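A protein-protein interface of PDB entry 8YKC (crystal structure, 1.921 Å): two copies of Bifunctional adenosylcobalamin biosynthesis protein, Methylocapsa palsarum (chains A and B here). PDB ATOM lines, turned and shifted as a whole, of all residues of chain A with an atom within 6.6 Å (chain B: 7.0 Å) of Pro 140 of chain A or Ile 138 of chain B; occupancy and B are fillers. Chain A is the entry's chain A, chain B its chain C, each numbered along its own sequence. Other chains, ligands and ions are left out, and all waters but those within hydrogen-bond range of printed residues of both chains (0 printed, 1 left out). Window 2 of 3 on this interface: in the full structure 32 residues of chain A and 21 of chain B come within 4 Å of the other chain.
The backbone NH (N) of Ala 136 of chain A sits at hydrogen-bond distance from the backbone carbonyl oxygen (O) of Ala 136 of chain B (2.9 Å). O of Ala 136 of chain B lies within hydrogen-bond range of N of Gly 135 of chain A, 3.2 Å away.
Of the 16 printed residues of chain A, 6 touch a printed residue of chain B. Printed residues of chain A that touch a printed residue of chain B: Glu 133, Val 134, Gly 135, Ala 136, Gly 137 and Pro 140. Hydrophobic or aromatic side chains of chain A within 4 Å of the printed part of chain B: Val 134, Ala 136 and Pro 140. Printed residues of chain B that touch a printed residue of chain A: Gly 135, Ala 136, Gly 137 and Ile 138. Among the printed residues, 9 pairs touch across the chains. Among the printed residues, no Asp or Glu carboxylate lies within 4 Å of a Lys or Arg side-chain nitrogen of the other chain.
Printed residues of chain B within 4 Å of Val 134 of chain A: Ala 136 (3.2 Å), Gly 137 (3.5 Å) and Ile 138 (3.9 Å). Of the printed residues of chain B, Gly 137 of chain A touches Ala 136. Val 134 of chain B touches none of the printed residues of chain A. Printed residues of chain A within 4 Å of Ala 136 of chain B: Glu 133, Val 134, Gly 135, Ala 136 and Gly 137. Printed residues of chain A within 4 Å of Ile 138 of chain B: Val 134 (3.9 Å) and Pro 140 (3.8 Å).
Val 134 of chain A touches Ala 136 of chain B, but with the chains exchanged Ala 136 of chain A does not touch Val 134 of chain B (7.8 Å). Val 134 of chain A touches Gly 137 of chain B, but with the chains exchanged Gly 137 of chain A does not touch Val 134 of chain B (7.6 Å). Gly 135 of chain A touches Ala 136 of chain B, but with the chains exchanged Ala 136 of chain A does not touch Gly 135 of chain B (7.1 Å). Pro 140 of chain A touches Ile 138 of chain B, but with the chains exchanged Ile 138 of chain A does not touch Pro 140 of chain B (10.2 Å). Positions printed for both chains: 134, 135, 136, 137, 138, 139, 140, 141 and 149.
Glu 133 of chain A touches Gly 135 of chain B. Glu 133 of chain A touches Ala 136 of chain B (O to CA, 3.6 Å). Val 134 of chain A touches Ala 136 of chain B. Gly 137 of chain B touches Val 134 of chain A. Val 134 of chain A touches Ile 138 of chain B (O to N, 3.9 Å). N of Gly 137 of chain A touches O of Ala 136 of chain B (3.9 Å). Pro 140 of chain A touches Ile 138 of chain B.
The backbone carbonyl oxygen (O) of Pro 140 of chain A is in hydrogen-bond range of the guanidinium group (NH1) of Arg 146 of chain A. O of Gly 137 of chain B sits at hydrogen-bond distance from NH2 of Arg 149 of chain B (3.0 Å). The backbone NH of Gly 135 of chain A lies within hydrogen-bond range of the side-chain carboxylate of Glu 133 of chain A. O of Gly 137 of chain A sits at hydrogen-bond distance from NH2 of Arg 149 of chain A, 2.9 Å away.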
ATOM      1  N   GLU A 133       9.018  35.689 -27.806  1.00  0.00           N
ATOM      2  CA  GLU A 133       8.744  35.218 -26.438  1.00  0.00           C
ATOM      3  C   GLU A 133       9.361  33.821 -26.306  1.00  0.00           C
ATOM      4  O   GLU A 133       9.019  32.963 -27.124  1.00  0.00           O
ATOM      5  CB  GLU A 133       7.234  35.205 -26.189  1.00  0.00           C
ATOM      6  CG  GLU A 133       6.881  34.668 -24.807  1.00  0.00           C
ATOM      7  CD  GLU A 133       7.448  35.518 -23.693  1.00  0.00           C
ATOM      8  OE1 GLU A 133       8.200  34.971 -22.851  1.00  0.00           O
ATOM      9  OE2 GLU A 133       7.183  36.740 -23.704  1.00  0.00           O
ATOM     10  N   VAL A 134      10.246  33.623 -25.325  1.00  0.00           N
ATOM     11  CA  VAL A 134      10.835  32.281 -25.036  1.00  0.00           C
ATOM     12  C   VAL A 134      10.639  31.885 -23.568  1.00  0.00           C
ATOM     13  O   VAL A 134      11.173  30.792 -23.183  1.00  0.00           O
ATOM     14  CB  VAL A 134      12.323  32.225 -25.431  1.00  0.00           C
ATOM     15  CG1 VAL A 134      12.536  32.603 -26.884  1.00  0.00           C
ATOM     16  CG2 VAL A 134      13.187  33.077 -24.538  1.00  0.00           C
ATOM     17  N   GLY A 135       9.791  32.607 -22.816  1.00  0.00           N
ATOM     18  CA  GLY A 135       9.676  32.479 -21.353  1.00  0.00           C
ATOM     19  C   GLY A 135       8.522  31.617 -20.864  1.00  0.00           C
ATOM     20  O   GLY A 135       8.464  31.425 -19.676  1.00  0.00           O
ATOM     21  N   ALA A 136       7.637  31.113 -21.735  1.00  0.00           N
ATOM     22  CA  ALA A 136       6.308  30.612 -21.315  1.00  0.00           C
ATOM     23  C   ALA A 136       6.262  29.082 -21.383  1.00  0.00           C
ATOM     24  O   ALA A 136       5.148  28.513 -21.357  1.00  0.00           O
ATOM     25  CB  ALA A 136       5.222  31.304 -22.124  1.00  0.00           C
ATOM     26  N   GLY A 137       7.431  28.439 -21.467  1.00  0.00           N
ATOM     27  CA  GLY A 137       7.629  26.979 -21.320  1.00  0.00           C
ATOM     28  C   GLY A 137       8.184  26.624 -19.939  1.00  0.00           C
ATOM     29  O   GLY A 137       8.182  27.490 -19.009  1.00  0.00           O
ATOM     30  N   ILE A 138       8.685  25.401 -19.800  1.00  0.00           N
ATOM     31  CA  ILE A 138       9.243  24.893 -18.510  1.00  0.00           C
ATOM     32  C   ILE A 138      10.677  25.391 -18.353  1.00  0.00           C
ATOM     33  O   ILE A 138      11.246  25.913 -19.355  1.00  0.00           O
ATOM     34  CB  ILE A 138       9.133  23.358 -18.455  1.00  0.00           C
ATOM     35  CG1 ILE A 138      10.043  22.670 -19.473  1.00  0.00           C
ATOM     36  CG2 ILE A 138       7.686  22.931 -18.612  1.00  0.00           C
ATOM     37  CD1 ILE A 138      10.318  21.224 -19.088  1.00  0.00           C
ATOM     38  N   VAL A 139      11.249  25.300 -17.144  1.00  0.00           N
ATOM     39  CA  VAL A 139      12.669  25.715 -16.931  1.00  0.00           C
ATOM     40  C   VAL A 139      13.555  24.760 -17.725  1.00  0.00           C
ATOM     41  O   VAL A 139      13.406  23.539 -17.602  1.00  0.00           O
ATOM     42  CB  VAL A 139      13.023  25.721 -15.429  1.00  0.00           C
ATOM     43  CG1 VAL A 139      14.515  25.874 -15.201  1.00  0.00           C
ATOM     44  CG2 VAL A 139      12.229  26.785 -14.686  1.00  0.00           C
ATOM     45  N   PRO A 140      14.462  25.255 -18.598  1.00  0.00           N
ATOM     46  CA  PRO A 140      15.362  24.358 -19.322  1.00  0.00           C
ATOM     47  C   PRO A 140      16.344  23.572 -18.428  1.00  0.00           C
ATOM     48  O   PRO A 140      16.733  24.064 -17.378  1.00  0.00           O
ATOM     49  CB  PRO A 140      16.159  25.262 -20.276  1.00  0.00           C
ATOM     50  CG  PRO A 140      15.509  26.648 -20.215  1.00  0.00           C
ATOM     51  CD  PRO A 140      14.591  26.662 -19.011  1.00  0.00           C
ATOM     52  N   ASP A 141      16.715  22.374 -18.886  1.00  0.00           N
ATOM     53  CA  ASP A 141      17.767  21.486 -18.314  1.00  0.00           C
ATOM     54  C   ASP A 141      19.126  22.177 -18.198  1.00  0.00           C
ATOM     55  O   ASP A 141      19.692  22.152 -17.094  1.00  0.00           O
ATOM     56  CB  ASP A 141      18.039  20.277 -19.212  1.00  0.00           C
ATOM     57  CG  ASP A 141      16.901  19.288 -19.307  1.00  0.00           C
ATOM     58  OD1 ASP A 141      16.092  19.229 -18.351  1.00  0.00           O
ATOM     59  OD2 ASP A 141      16.840  18.576 -20.335  1.00  0.00           O
ATOM     60  N   ASN A 142      19.662  22.730 -19.288  1.00  0.00           N
ATOM     61  CA  ASN A 142      21.086  23.157 -19.349  1.00  0.00           C
ATOM     62  C   ASN A 142      21.234  24.649 -18.994  1.00  0.00           C
ATOM     63  O   ASN A 142      20.235  25.419 -19.041  1.00  0.00           O
ATOM     64  CB  ASN A 142      21.740  22.763 -20.673  1.00  0.00           C
ATOM     65  CG  ASN A 142      21.299  23.592 -21.859  1.00  0.00           C
ATOM     66  OD1 ASN A 142      21.990  24.523 -22.264  1.00  0.00           O
ATOM     67  ND2 ASN A 142      20.165  23.248 -22.437  1.00  0.00           N
ATOM     68  N   ALA A 143      22.455  25.043 -18.637  1.00  0.00           N
ATOM     69  CA  ALA A 143      22.773  26.367 -18.071  1.00  0.00           C
ATOM     70  C   ALA A 143      22.700  27.416 -19.174  1.00  0.00           C
ATOM     71  O   ALA A 143      22.204  28.507 -18.892  1.00  0.00           O
ATOM     72  CB  ALA A 143      24.126  26.351 -17.415  1.00  0.00           C
ATOM     73  N   ALA A 145      20.889  27.409 -22.002  1.00  0.00           N
ATOM     74  CA  ALA A 145      19.463  27.597 -22.350  1.00  0.00           C
ATOM     75  C   ALA A 145      18.789  28.486 -21.293  1.00  0.00           C
ATOM     76  O   ALA A 145      18.019  29.394 -21.690  1.00  0.00           O
ATOM     77  CB  ALA A 145      18.763  26.271 -22.492  1.00  0.00           C
ATOM     78  N   ARG A 146      19.072  28.245 -20.004  1.00  0.00           N
ATOM     79  CA  ARG A 146      18.515  29.038 -18.876  1.00  0.00           C
ATOM     80  C   ARG A 146      19.027  30.485 -18.964  1.00  0.00           C
ATOM     81  O   ARG A 146      18.222  31.407 -18.707  1.00  0.00           O
ATOM     82  CB  ARG A 146      18.832  28.387 -17.523  1.00  0.00           C
ATOM     83  CG  ARG A 146      17.850  27.301 -17.114  1.00  0.00           C
ATOM     84  CD  ARG A 146      17.839  27.039 -15.621  1.00  0.00           C
ATOM     85  NE  ARG A 146      19.185  26.706 -15.194  1.00  0.00           N
ATOM     86  CZ  ARG A 146      19.761  25.522 -15.330  1.00  0.00           C
ATOM     87  NH1 ARG A 146      19.107  24.512 -15.878  1.00  0.00           N
ATOM     88  NH2 ARG A 146      21.002  25.347 -14.906  1.00  0.00           N
ATOM     89  N   ALA A 147      20.295  30.694 -19.312  1.00  0.00           N
ATOM     90  CA  ALA A 147      20.913  32.038 -19.372  1.00  0.00           C
ATOM     91  C   ALA A 147      20.287  32.776 -20.563  1.00  0.00           C
ATOM     92  O   ALA A 147      20.030  33.989 -20.454  1.00  0.00           O
ATOM     93  CB  ALA A 147      22.430  31.962 -19.513  1.00  0.00           C
ATOM     94  N   PHE A 148      20.066  32.060 -21.660  1.00  0.00           N
ATOM     95  CA  PHE A 148      19.467  32.625 -22.887  1.00  0.00           C
ATOM     96  C   PHE A 148      18.029  33.053 -22.584  1.00  0.00           C
ATOM     97  O   PHE A 148      17.641  34.172 -22.940  1.00  0.00           O
ATOM     98  CB  PHE A 148      19.543  31.657 -24.058  1.00  0.00           C
ATOM     99  CG  PHE A 148      18.938  32.232 -25.302  1.00  0.00           C
ATOM    100  CD1 PHE A 148      19.624  33.198 -26.017  1.00  0.00           C
ATOM    101  CD2 PHE A 148      17.643  31.919 -25.673  1.00  0.00           C
ATOM    102  CE1 PHE A 148      19.055  33.778 -27.141  1.00  0.00           C
ATOM    103  CE2 PHE A 148      17.061  32.530 -26.778  1.00  0.00           C
ATOM    104  CZ  PHE A 148      17.782  33.440 -27.521  1.00  0.00           C
ATOM    105  N   ARG A 149      17.261  32.184 -21.953  1.00  0.00           N
ATOM    106  CA  ARG A 149      15.821  32.432 -21.697  1.00  0.00           C
ATOM    107  C   ARG A 149      15.691  33.693 -20.847  1.00  0.00           C
ATOM    108  O   ARG A 149      14.902  34.567 -21.152  1.00  0.00           O
ATOM    109  CB  ARG A 149      15.247  31.175 -21.042  1.00  0.00           C
ATOM    110  CG  ARG A 149      13.769  31.226 -20.700  1.00  0.00           C
ATOM    111  CD  ARG A 149      13.549  29.928 -19.963  1.00  0.00           C
ATOM    112  NE  ARG A 149      12.231  29.537 -19.577  1.00  0.00           N
ATOM    113  CZ  ARG A 149      11.783  29.411 -18.331  1.00  0.00           C
ATOM    114  NH1 ARG A 149      12.541  29.674 -17.279  1.00  0.00           N
ATOM    115  NH2 ARG A 149      10.574  28.937 -18.155  1.00  0.00           N
ATOM    116  N   VAL B 134       2.380  26.253 -28.831  1.00  0.00           N
ATOM    117  CA  VAL B 134       3.609  25.492 -28.435  1.00  0.00           C
ATOM    118  C   VAL B 134       4.880  26.279 -28.797  1.00  0.00           C
ATOM    119  O   VAL B 134       5.976  25.723 -28.646  1.00  0.00           O
ATOM    120  CB  VAL B 134       3.663  24.084 -29.067  1.00  0.00           C
ATOM    121  CG1 VAL B 134       2.453  23.226 -28.742  1.00  0.00           C
ATOM    122  CG2 VAL B 134       3.893  24.153 -30.555  1.00  0.00           C
ATOM    123  N   GLY B 135       4.781  27.528 -29.259  1.00  0.00           N
ATOM    124  CA  GLY B 135       5.969  28.242 -29.745  1.00  0.00           C
ATOM    125  C   GLY B 135       6.615  29.200 -28.748  1.00  0.00           C
ATOM    126  O   GLY B 135       7.540  29.900 -29.176  1.00  0.00           O
ATOM    127  N   ALA B 136       6.140  29.325 -27.504  1.00  0.00           N
ATOM    128  CA  ALA B 136       6.553  30.455 -26.626  1.00  0.00           C
ATOM    129  C   ALA B 136       7.600  30.005 -25.592  1.00  0.00           C
ATOM    130  O   ALA B 136       7.833  30.734 -24.609  1.00  0.00           O
ATOM    131  CB  ALA B 136       5.350  31.086 -25.988  1.00  0.00           C
ATOM    132  N   GLY B 137       8.239  28.862 -25.836  1.00  0.00           N
ATOM    133  CA  GLY B 137       9.428  28.407 -25.102  1.00  0.00           C
ATOM    134  C   GLY B 137      10.652  28.396 -25.995  1.00  0.00           C
ATOM    135  O   GLY B 137      10.654  29.029 -27.048  1.00  0.00           O
ATOM    136  N   ILE B 138      11.703  27.742 -25.527  1.00  0.00           N
ATOM    137  CA  ILE B 138      13.045  27.724 -26.194  1.00  0.00           C
ATOM    138  C   ILE B 138      13.003  26.792 -27.418  1.00  0.00           C
ATOM    139  O   ILE B 138      12.010  26.054 -27.581  1.00  0.00           O
ATOM    140  CB  ILE B 138      14.124  27.335 -25.152  1.00  0.00           C
ATOM    141  CG1 ILE B 138      13.917  25.912 -24.631  1.00  0.00           C
ATOM    142  CG2 ILE B 138      14.181  28.372 -24.040  1.00  0.00           C
ATOM    143  CD1 ILE B 138      15.149  25.313 -23.949  1.00  0.00           C
ATOM    144  N   VAL B 139      13.986  26.897 -28.313  1.00  0.00           N
ATOM    145  CA  VAL B 139      14.087  26.031 -29.526  1.00  0.00           C
ATOM    146  C   VAL B 139      14.385  24.620 -29.023  1.00  0.00           C
ATOM    147  O   VAL B 139      15.347  24.437 -28.258  1.00  0.00           O
ATOM    148  CB  VAL B 139      15.178  26.513 -30.499  1.00  0.00           C
ATOM    149  CG1 VAL B 139      15.340  25.548 -31.663  1.00  0.00           C
ATOM    150  CG2 VAL B 139      14.962  27.934 -30.999  1.00  0.00           C
ATOM    151  N   PRO B 140      13.524  23.618 -29.323  1.00  0.00           N
ATOM    152  CA  PRO B 140      13.782  22.243 -28.906  1.00  0.00           C
ATOM    153  C   PRO B 140      15.068  21.654 -29.505  1.00  0.00           C
ATOM    154  O   PRO B 140      15.448  22.001 -30.606  1.00  0.00           O
ATOM    155  CB  PRO B 140      12.594  21.428 -29.425  1.00  0.00           C
ATOM    156  CG  PRO B 140      11.504  22.448 -29.741  1.00  0.00           C
ATOM    157  CD  PRO B 140      12.207  23.769 -29.967  1.00  0.00           C
ATOM    158  N   ASP B 141      15.679  20.723 -28.769  1.00  0.00           N
ATOM    159  CA  ASP B 141      17.005  20.155 -29.138  1.00  0.00           C
ATOM    160  C   ASP B 141      16.829  19.102 -30.239  1.00  0.00           C
ATOM    161  O   ASP B 141      17.730  19.016 -31.080  1.00  0.00           O
ATOM    162  CB  ASP B 141      17.749  19.617 -27.918  1.00  0.00           C
ATOM    163  CG  ASP B 141      19.199  20.067 -27.901  1.00  0.00           C
ATOM    164  OD1 ASP B 141      20.007  19.494 -28.675  1.00  0.00           O
ATOM    165  OD2 ASP B 141      19.500  21.023 -27.142  1.00  0.00           O
ATOM    166  N   ARG B 149       6.752  21.992 -33.603  1.00  0.00           N
ATOM    167  CA  ARG B 149       6.688  23.412 -33.160  1.00  0.00           C
ATOM    168  C   ARG B 149       6.415  24.341 -34.351  1.00  0.00           C
ATOM    169  O   ARG B 149       5.512  25.159 -34.246  1.00  0.00           O
ATOM    170  CB  ARG B 149       8.000  23.805 -32.476  1.00  0.00           C
ATOM    171  CG  ARG B 149       7.978  25.170 -31.793  1.00  0.00           C
ATOM    172  CD  ARG B 149       9.268  25.264 -31.003  1.00  0.00           C
ATOM    173  NE  ARG B 149       9.640  26.508 -30.315  1.00  0.00           N
ATOM    174  CZ  ARG B 149      10.562  27.349 -30.739  1.00  0.00           C
ATOM    175  NH1 ARG B 149      11.148  27.170 -31.910  1.00  0.00           N
ATOM    176  NH2 ARG B 149      10.903  28.387 -29.987  1.00  0.00           N
